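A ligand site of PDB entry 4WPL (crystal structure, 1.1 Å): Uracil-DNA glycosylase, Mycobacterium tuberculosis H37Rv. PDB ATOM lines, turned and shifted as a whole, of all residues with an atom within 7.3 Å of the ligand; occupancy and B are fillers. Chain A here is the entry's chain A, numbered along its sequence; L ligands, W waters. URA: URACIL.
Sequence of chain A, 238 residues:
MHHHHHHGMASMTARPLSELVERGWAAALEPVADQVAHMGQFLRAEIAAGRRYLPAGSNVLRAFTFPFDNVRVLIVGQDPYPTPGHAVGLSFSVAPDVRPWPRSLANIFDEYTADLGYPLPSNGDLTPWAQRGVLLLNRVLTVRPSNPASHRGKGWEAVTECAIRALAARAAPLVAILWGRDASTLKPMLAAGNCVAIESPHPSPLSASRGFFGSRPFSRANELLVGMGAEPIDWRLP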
ATOM      1  N   VAL A  76     -22.380   0.577   9.601  1.00  0.00           N
ATOM      2  CA  VAL A  76     -22.875  -0.374   8.656  1.00  0.00           C
ATOM      3  C   VAL A  76     -22.055  -0.338   7.404  1.00  0.00           C
ATOM      4  O   VAL A  76     -21.941   0.697   6.745  1.00  0.00           O
ATOM      5  CB  VAL A  76     -24.363  -0.153   8.311  1.00  0.00           C
ATOM      6  CG1 VAL A  76     -24.899  -1.334   7.519  1.00  0.00           C
ATOM      7  CG2 VAL A  76     -25.207   0.016   9.564  1.00  0.00           C
ATOM      8  N   GLY A  77     -21.468  -1.481   7.037  1.00  0.00           N
ATOM      9  CA  GLY A  77     -20.896  -1.671   5.744  1.00  0.00           C
ATOM     10  C   GLY A  77     -21.755  -2.482   4.807  1.00  0.00           C
ATOM     11  O   GLY A  77     -22.969  -2.600   4.977  1.00  0.00           O
ATOM     12  N   GLN A  78     -21.107  -3.030   3.806  1.00  0.00           N
ATOM     13  CA  GLN A  78     -21.777  -3.743   2.721  1.00  0.00           C
ATOM     14  C   GLN A  78     -21.985  -5.218   3.005  1.00  0.00           C
ATOM     15  O   GLN A  78     -23.123  -5.693   3.098  1.00  0.00           O
ATOM     16  CB  GLN A  78     -21.004  -3.543   1.409  1.00  0.00           C
ATOM     17  CG  GLN A  78     -21.635  -4.291   0.259  1.00  0.00           C
ATOM     18  CD  GLN A  78     -20.900  -4.100  -1.042  1.00  0.00           C
ATOM     19  OE1 GLN A  78     -21.040  -3.058  -1.695  1.00  0.00           O
ATOM     20  NE2 GLN A  78     -20.118  -5.090  -1.433  1.00  0.00           N
ATOM     21  N   ASP A  79     -20.893  -5.966   3.127  1.00  0.00           N
ATOM     22  CA  ASP A  79     -20.895  -7.398   3.306  1.00  0.00           C
ATOM     23  C   ASP A  79     -19.528  -7.795   3.826  1.00  0.00           C
ATOM     24  O   ASP A  79     -18.605  -6.976   3.852  1.00  0.00           O
ATOM     25  CB  ASP A  79     -21.329  -8.124   2.009  1.00  0.00           C
ATOM     26  CG  ASP A  79     -20.353  -8.094   0.870  1.00  0.00           C
ATOM     27  OD1 ASP A  79     -19.600  -7.114   0.702  1.00  0.00           O
ATOM     28  OD2 ASP A  79     -20.391  -9.099   0.094  1.00  0.00           O
ATOM     29  N   PRO A  80     -19.378  -9.037   4.273  1.00  0.00           N
ATOM     30  CA  PRO A  80     -18.107  -9.411   4.946  1.00  0.00           C
ATOM     31  C   PRO A  80     -16.925  -9.416   4.010  1.00  0.00           C
ATOM     32  O   PRO A  80     -17.042  -9.560   2.796  1.00  0.00           O
ATOM     33  CB  PRO A  80     -18.390 -10.800   5.494  1.00  0.00           C
ATOM     34  CG  PRO A  80     -19.903 -10.836   5.677  1.00  0.00           C
ATOM     35  CD  PRO A  80     -20.399 -10.089   4.459  1.00  0.00           C
ATOM     36  N   TYR A  81     -15.746  -9.416   4.604  1.00  0.00           N
ATOM     37  CA  TYR A  81     -14.516  -9.593   3.827  1.00  0.00           C
ATOM     38  C   TYR A  81     -14.606 -10.885   3.021  1.00  0.00           C
ATOM     39  O   TYR A  81     -14.995 -11.906   3.532  1.00  0.00           O
ATOM     40  CB  TYR A  81     -13.299  -9.683   4.684  1.00  0.00           C
ATOM     41  CG  TYR A  81     -12.890  -8.411   5.367  1.00  0.00           C
ATOM     42  CD1 TYR A  81     -12.524  -7.302   4.634  1.00  0.00           C
ATOM     43  CD2 TYR A  81     -12.852  -8.289   6.750  1.00  0.00           C
ATOM     44  CE1 TYR A  81     -12.139  -6.110   5.251  1.00  0.00           C
ATOM     45  CE2 TYR A  81     -12.461  -7.128   7.381  1.00  0.00           C
ATOM     46  CZ  TYR A  81     -12.110  -6.016   6.635  1.00  0.00           C
ATOM     47  OH  TYR A  81     -11.721  -4.849   7.195  1.00  0.00           O
ATOM     48  N   PRO A  82     -14.125 -10.852   1.760  1.00  0.00           N
ATOM     49  CA  PRO A  82     -14.232 -12.038   0.908  1.00  0.00           C
ATOM     50  C   PRO A  82     -13.087 -13.018   1.022  1.00  0.00           C
ATOM     51  O   PRO A  82     -13.165 -14.124   0.485  1.00  0.00           O
ATOM     52  CB  PRO A  82     -14.283 -11.401  -0.501  1.00  0.00           C
ATOM     53  CG  PRO A  82     -13.403 -10.170  -0.359  1.00  0.00           C
ATOM     54  CD  PRO A  82     -13.841  -9.630   0.978  1.00  0.00           C
ATOM     55  N   ALA A  87     -12.935 -12.268   7.620  1.00  0.00           N
ATOM     56  CA  ALA A  87     -14.224 -11.937   8.260  1.00  0.00           C
ATOM     57  C   ALA A  87     -14.411 -12.671   9.558  1.00  0.00           C
ATOM     58  O   ALA A  87     -14.204 -13.907   9.619  1.00  0.00           O
ATOM     59  CB  ALA A  87     -15.342 -12.272   7.327  1.00  0.00           C
ATOM     60  N   VAL A  88     -14.868 -11.936  10.563  1.00  0.00           N
ATOM     61  CA  VAL A  88     -15.069 -12.518  11.927  1.00  0.00           C
ATOM     62  C   VAL A  88     -16.445 -12.220  12.460  1.00  0.00           C
ATOM     63  O   VAL A  88     -16.715 -12.513  13.626  1.00  0.00           O
ATOM     64  CB  VAL A  88     -13.990 -12.013  12.927  1.00  0.00           C
ATOM     65  CG1 VAL A  88     -12.612 -12.348  12.473  1.00  0.00           C
ATOM     66  CG2 VAL A  88     -14.136 -10.498  13.164  1.00  0.00           C
ATOM     67  N   GLY A  89     -17.373 -11.667  11.641  1.00  0.00           N
ATOM     68  CA  GLY A  89     -18.739 -11.428  12.118  1.00  0.00           C
ATOM     69  C   GLY A  89     -18.972 -10.086  12.778  1.00  0.00           C
ATOM     70  O   GLY A  89     -20.064  -9.799  13.196  1.00  0.00           O
ATOM     71  N   LEU A  90     -17.918  -9.286  12.911  1.00  0.00           N
ATOM     72  CA  LEU A  90     -17.999  -7.876  13.276  1.00  0.00           C
ATOM     73  C   LEU A  90     -17.487  -7.122  12.080  1.00  0.00           C
ATOM     74  O   LEU A  90     -16.376  -7.385  11.617  1.00  0.00           O
ATOM     75  CB  LEU A  90     -17.146  -7.589  14.508  1.00  0.00           C
ATOM     76  CG  LEU A  90     -17.596  -8.316  15.764  1.00  0.00           C
ATOM     77  CD1 LEU A  90     -16.572  -8.060  16.896  1.00  0.00           C
ATOM     78  CD2 LEU A  90     -19.002  -7.974  16.190  1.00  0.00           C
ATOM     79  N   SER A  91     -18.304  -6.211  11.539  1.00  0.00           N
ATOM     80  CA  SER A  91     -17.908  -5.604  10.284  1.00  0.00           C
ATOM     81  C   SER A  91     -16.547  -4.919  10.433  1.00  0.00           C
ATOM     82  O   SER A  91     -16.241  -4.287  11.428  1.00  0.00           O
ATOM     83  CB  SER A  91     -18.986  -4.684   9.758  1.00  0.00           C
ATOM     84  OG  SER A  91     -19.170  -3.565  10.592  1.00  0.00           O
ATOM     85  N   PHE A  92     -15.731  -5.120   9.410  1.00  0.00           N
ATOM     86  CA  PHE A  92     -14.420  -4.563   9.211  1.00  0.00           C
ATOM     87  C   PHE A  92     -13.320  -5.117  10.113  1.00  0.00           C
ATOM     88  O   PHE A  92     -12.145  -4.910   9.857  1.00  0.00           O
ATOM     89  CB  PHE A  92     -14.418  -3.028   9.206  1.00  0.00           C
ATOM     90  CG  PHE A  92     -15.311  -2.466   8.130  1.00  0.00           C
ATOM     91  CD1 PHE A  92     -14.900  -2.437   6.823  1.00  0.00           C
ATOM     92  CD2 PHE A  92     -16.583  -2.065   8.412  1.00  0.00           C
ATOM     93  CE1 PHE A  92     -15.721  -1.922   5.837  1.00  0.00           C
ATOM     94  CE2 PHE A  92     -17.426  -1.606   7.422  1.00  0.00           C
ATOM     95  CZ  PHE A  92     -16.981  -1.481   6.131  1.00  0.00           C
ATOM     96  N   SER A  93     -13.689  -5.812  11.200  1.00  0.00           N
ATOM     97  CA  SER A  93     -12.703  -6.303  12.134  1.00  0.00           C
ATOM     98  C   SER A  93     -11.962  -7.497  11.576  1.00  0.00           C
ATOM     99  O   SER A  93     -12.506  -8.282  10.784  1.00  0.00           O
ATOM    100  CB  SER A  93     -13.474  -6.703  13.410  1.00  0.00           C
ATOM    101  OG  SER A  93     -12.584  -6.848  14.486  1.00  0.00           O
ATOM    102  N   PRO A 102      -6.660  -5.866   5.656  1.00  0.00           N
ATOM    103  CA  PRO A 102      -7.459  -5.585   4.471  1.00  0.00           C
ATOM    104  C   PRO A 102      -7.351  -4.109   4.086  1.00  0.00           C
ATOM    105  O   PRO A 102      -7.293  -3.240   4.959  1.00  0.00           O
ATOM    106  CB  PRO A 102      -8.860  -5.950   4.901  1.00  0.00           C
ATOM    107  CG  PRO A 102      -8.681  -6.941   5.955  1.00  0.00           C
ATOM    108  CD  PRO A 102      -7.450  -6.542   6.723  1.00  0.00           C
ATOM    109  N   SER A 104      -9.654  -1.971   2.996  1.00  0.00           N
ATOM    110  CA  SER A 104     -10.607  -1.041   3.554  1.00  0.00           C
ATOM    111  C   SER A 104     -10.331  -0.731   5.008  1.00  0.00           C
ATOM    112  O   SER A 104     -10.600   0.382   5.472  1.00  0.00           O
ATOM    113  CB  SER A 104     -12.041  -1.562   3.389  1.00  0.00           C
ATOM    114  OG  SER A 104     -12.217  -2.797   4.081  1.00  0.00           O
ATOM    115  N   LEU A 105      -9.830  -1.701   5.752  1.00  0.00           N
ATOM    116  CA  LEU A 105      -9.449  -1.453   7.154  1.00  0.00           C
ATOM    117  C   LEU A 105      -8.285  -0.489   7.240  1.00  0.00           C
ATOM    118  O   LEU A 105      -8.265   0.410   8.085  1.00  0.00           O
ATOM    119  CB  LEU A 105      -9.159  -2.740   7.886  1.00  0.00           C
ATOM    120  CG  LEU A 105      -8.936  -2.600   9.385  1.00  0.00           C
ATOM    121  CD1 LEU A 105     -10.110  -1.965  10.079  1.00  0.00           C
ATOM    122  CD2 LEU A 105      -8.636  -3.959   9.970  1.00  0.00           C
ATOM    123  N   ILE A 108      -9.854   2.800   6.812  1.00  0.00           N
ATOM    124  CA  ILE A 108     -10.532   3.181   8.026  1.00  0.00           C
ATOM    125  C   ILE A 108      -9.521   3.726   9.049  1.00  0.00           C
ATOM    126  O   ILE A 108      -9.768   4.758   9.678  1.00  0.00           O
ATOM    127  CB  ILE A 108     -11.343   2.051   8.607  1.00  0.00           C
ATOM    128  CG1 ILE A 108     -12.540   1.718   7.700  1.00  0.00           C
ATOM    129  CG2 ILE A 108     -11.813   2.324  10.033  1.00  0.00           C
ATOM    130  CD1 ILE A 108     -13.152   0.374   7.987  1.00  0.00           C
ATOM    131  N   LEU A 136     -21.119  -3.251  14.926  1.00  0.00           N
ATOM    132  CA  LEU A 136     -20.345  -3.388  13.712  1.00  0.00           C
ATOM    133  C   LEU A 136     -21.077  -4.317  12.744  1.00  0.00           C
ATOM    134  O   LEU A 136     -20.874  -5.526  12.712  1.00  0.00           O
ATOM    135  CB  LEU A 136     -18.945  -3.906  14.064  1.00  0.00           C
ATOM    136  CG  LEU A 136     -18.111  -2.959  14.913  1.00  0.00           C
ATOM    137  CD1 LEU A 136     -16.862  -3.647  15.400  1.00  0.00           C
ATOM    138  CD2 LEU A 136     -17.743  -1.698  14.125  1.00  0.00           C
ATOM    139  N   LEU A 137     -22.033  -3.699  12.030  1.00  0.00           N
ATOM    140  CA  LEU A 137     -22.953  -4.418  11.150  1.00  0.00           C
ATOM    141  C   LEU A 137     -22.533  -4.335   9.700  1.00  0.00           C
ATOM    142  O   LEU A 137     -21.813  -3.410   9.301  1.00  0.00           O
ATOM    143  CB  LEU A 137     -24.347  -3.863  11.349  1.00  0.00           C
ATOM    144  CG  LEU A 137     -25.544  -4.709  10.956  1.00  0.00           C
ATOM    145  CD1 LEU A 137     -25.564  -6.056  11.693  1.00  0.00           C
ATOM    146  CD2 LEU A 137     -26.813  -3.947  11.204  1.00  0.00           C
ATOM    147  N   ASN A 138     -23.015  -5.262   8.895  1.00  0.00           N
ATOM    148  CA  ASN A 138     -23.040  -5.142   7.439  1.00  0.00           C
ATOM    149  C   ASN A 138     -24.492  -5.249   6.977  1.00  0.00           C
ATOM    150  O   ASN A 138     -25.299  -5.919   7.634  1.00  0.00           O
ATOM    151  CB  ASN A 138     -22.216  -6.230   6.788  1.00  0.00           C
ATOM    152  CG  ASN A 138     -20.733  -5.975   6.867  1.00  0.00           C
ATOM    153  OD1 ASN A 138     -20.274  -4.883   6.505  1.00  0.00           O
ATOM    154  ND2 ASN A 138     -19.967  -6.949   7.313  1.00  0.00           N
ATOM    155  N   ARG A 139     -24.796  -4.695   5.819  1.00  0.00           N
ATOM    156  CA  ARG A 139     -26.143  -4.812   5.302  1.00  0.00           C
ATOM    157  C   ARG A 139     -26.507  -6.275   4.985  1.00  0.00           C
ATOM    158  O   ARG A 139     -27.638  -6.706   5.155  1.00  0.00           O
ATOM    159  CB  ARG A 139     -26.282  -3.957   4.039  1.00  0.00           C
ATOM    160  CG  ARG A 139     -27.702  -3.730   3.550  1.00  0.00           C
ATOM    161  CD  ARG A 139     -28.491  -2.825   4.489  1.00  0.00           C
ATOM    162  NE  ARG A 139     -29.743  -2.400   3.912  1.00  0.00           N
ATOM    163  CZ  ARG A 139     -30.896  -3.036   4.012  1.00  0.00           C
ATOM    164  NH1 ARG A 139     -31.059  -4.038   4.865  1.00  0.00           N
ATOM    165  NH2 ARG A 139     -31.917  -2.606   3.338  1.00  0.00           N
ATOM    166  N   VAL A 140     -25.485  -7.022   4.530  1.00  0.00           N
ATOM    167  CA  VAL A 140     -25.574  -8.446   4.211  1.00  0.00           C
ATOM    168  C   VAL A 140     -24.553  -9.169   5.052  1.00  0.00           C
ATOM    169  O   VAL A 140     -23.419  -8.693   5.171  1.00  0.00           O
ATOM    170  CB  VAL A 140     -25.338  -8.619   2.687  1.00  0.00           C
ATOM    171  CG1 VAL A 140     -25.046 -10.027   2.261  1.00  0.00           C
ATOM    172  CG2 VAL A 140     -26.567  -8.052   1.955  1.00  0.00           C
ATOM    173  N   TRP A 179     -21.717   3.376   5.531  1.00  0.00           N
ATOM    174  CA  TRP A 179     -20.609   3.399   4.562  1.00  0.00           C
ATOM    175  C   TRP A 179     -21.018   2.678   3.299  1.00  0.00           C
ATOM    176  O   TRP A 179     -21.128   1.421   3.294  1.00  0.00           O
ATOM    177  CB  TRP A 179     -19.373   2.773   5.197  1.00  0.00           C
ATOM    178  CG  TRP A 179     -18.666   3.637   6.176  1.00  0.00           C
ATOM    179  CD1 TRP A 179     -18.715   4.994   6.271  1.00  0.00           C
ATOM    180  CD2 TRP A 179     -17.781   3.189   7.199  1.00  0.00           C
ATOM    181  NE1 TRP A 179     -17.924   5.412   7.290  1.00  0.00           N
ATOM    182  CE2 TRP A 179     -17.340   4.339   7.877  1.00  0.00           C
ATOM    183  CE3 TRP A 179     -17.297   1.969   7.606  1.00  0.00           C
ATOM    184  CZ2 TRP A 179     -16.440   4.284   8.964  1.00  0.00           C
ATOM    185  CZ3 TRP A 179     -16.441   1.893   8.659  1.00  0.00           C
ATOM    186  CH2 TRP A 179     -15.999   3.021   9.332  1.00  0.00           C
ATOM    187  N   HIS A 202     -17.936   4.394   0.864  1.00  0.00           N
ATOM    188  CA  HIS A 202     -17.361   3.267   1.582  1.00  0.00           C
ATOM    189  C   HIS A 202     -15.834   3.372   1.593  1.00  0.00           C
ATOM    190  O   HIS A 202     -15.224   3.906   0.655  1.00  0.00           O
ATOM    191  CB  HIS A 202     -17.859   2.019   0.881  1.00  0.00           C
ATOM    192  CG  HIS A 202     -17.553   0.702   1.514  1.00  0.00           C
ATOM    193  ND1 HIS A 202     -16.317   0.143   1.409  1.00  0.00           N
ATOM    194  CD2 HIS A 202     -18.366  -0.175   2.157  1.00  0.00           C
ATOM    195  CE1 HIS A 202     -16.382  -1.046   1.966  1.00  0.00           C
ATOM    196  NE2 HIS A 202     -17.601  -1.261   2.444  1.00  0.00           N
ATOM    197  N   PRO A 203     -15.162   2.816   2.625  1.00  0.00           N
ATOM    198  CA  PRO A 203     -13.708   2.861   2.699  1.00  0.00           C
ATOM    199  C   PRO A 203     -12.964   1.957   1.748  1.00  0.00           C
ATOM    200  O   PRO A 203     -11.718   2.011   1.720  1.00  0.00           O
ATOM    201  CB  PRO A 203     -13.421   2.567   4.175  1.00  0.00           C
ATOM    202  CG  PRO A 203     -14.587   1.701   4.575  1.00  0.00           C
ATOM    203  CD  PRO A 203     -15.746   2.324   3.900  1.00  0.00           C
ATOM    204  N   SER A 204     -13.645   1.097   0.994  1.00  0.00           N
ATOM    205  CA  SER A 204     -13.001   0.350  -0.049  1.00  0.00           C
ATOM    206  C   SER A 204     -12.144   1.266  -0.923  1.00  0.00           C
ATOM    207  O   SER A 204     -12.571   2.361  -1.257  1.00  0.00           O
ATOM    208  CB  SER A 204     -14.094  -0.249  -0.953  1.00  0.00           C
ATOM    209  OG  SER A 204     -13.502  -0.760  -2.122  1.00  0.00           O
HETATM  210  N1  URA L   1     -16.304  -4.527   3.702  1.00  0.00           N
HETATM  211  C2  URA L   1     -17.480  -4.312   4.297  1.00  0.00           C
HETATM  212  O2  URA L   1     -18.368  -3.588   3.803  1.00  0.00           O
HETATM  213  N3  URA L   1     -17.665  -4.895   5.526  1.00  0.00           N
HETATM  214  C4  URA L   1     -16.778  -5.741   6.081  1.00  0.00           C
HETATM  215  O4  URA L   1     -17.103  -6.325   7.147  1.00  0.00           O
HETATM  216  C5  URA L   1     -15.541  -5.913   5.431  1.00  0.00           C
HETATM  217  C6  URA L   1     -15.345  -5.321   4.237  1.00  0.00           C
HETATM  218  O   HOH W   1     -16.111  -8.877   7.553  1.00  0.00           O
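C of Gly 77 touches O2 of the ligand, 3.7 Å away. Pro 80 touches the ligand. Tyr 81 touches the ligand. CA of Ser 91 touches O4 of the ligand, 3.3 Å away. Nine residues have an atom within 4 Å of the ligand: Gly 77, Gln 78, Asp 79, Pro 80, Tyr 81, Ser 91, Phe 92, Asn 138 and His 202.
A ring nitrogen (NE2) of His 202 lies within hydrogen-bond range of an oxygen (O2) of the ligand, at 2.8 Å. The side-chain amide oxygen (OD1) of Asn 138 is in hydrogen-bond range of a nitrogen (N3) of the ligand (2.8 Å). O of Asp 79 lies within hydrogen-bond range of N3 of the ligand, at 2.8 Å. The backbone NH (N) of Phe 92 is in hydrogen-bond range of an oxygen (O4) of the ligand. The backbone NH (N) of Gln 78 sits at hydrogen-bond distance from an oxygen (O2) of the ligand, 2.8 Å away.
Water W1 bridges an oxygen (O4) of the ligand and the backbone NH of Tyr 81.
N of Val 140 lies within hydrogen-bond range of O of Gln 78. The backbone NH (N) of Ser 204 lies within hydrogen-bond range of a ring nitrogen (ND1) of His 202, 2.9 Å away. The side-chain hydroxyl of Ser 91 lies within hydrogen-bond range of the backbone carbonyl oxygen of Leu 137. The backbone NH of Gly 77 sits at hydrogen-bond distance from the backbone carbonyl oxygen of Leu 137, 3.0 Å away. The backbone NH of Ser 91 sits at hydrogen-bond distance from the backbone carbonyl oxygen of Leu 136 (2.9 Å). The side-chain amide oxygen (OD1) of Asn 138 sits at hydrogen-bond distance from the backbone NH (N) of Gln 78. The backbone carbonyl oxygen of Phe 92 lies within hydrogen-bond range of the side-chain hydroxyl of Tyr 81, at 2.7 Å. The side-chain amide nitrogen of Gln 78 sits at hydrogen-bond distance from the side-chain carboxylate of Asp 79, at 3.0 Å.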
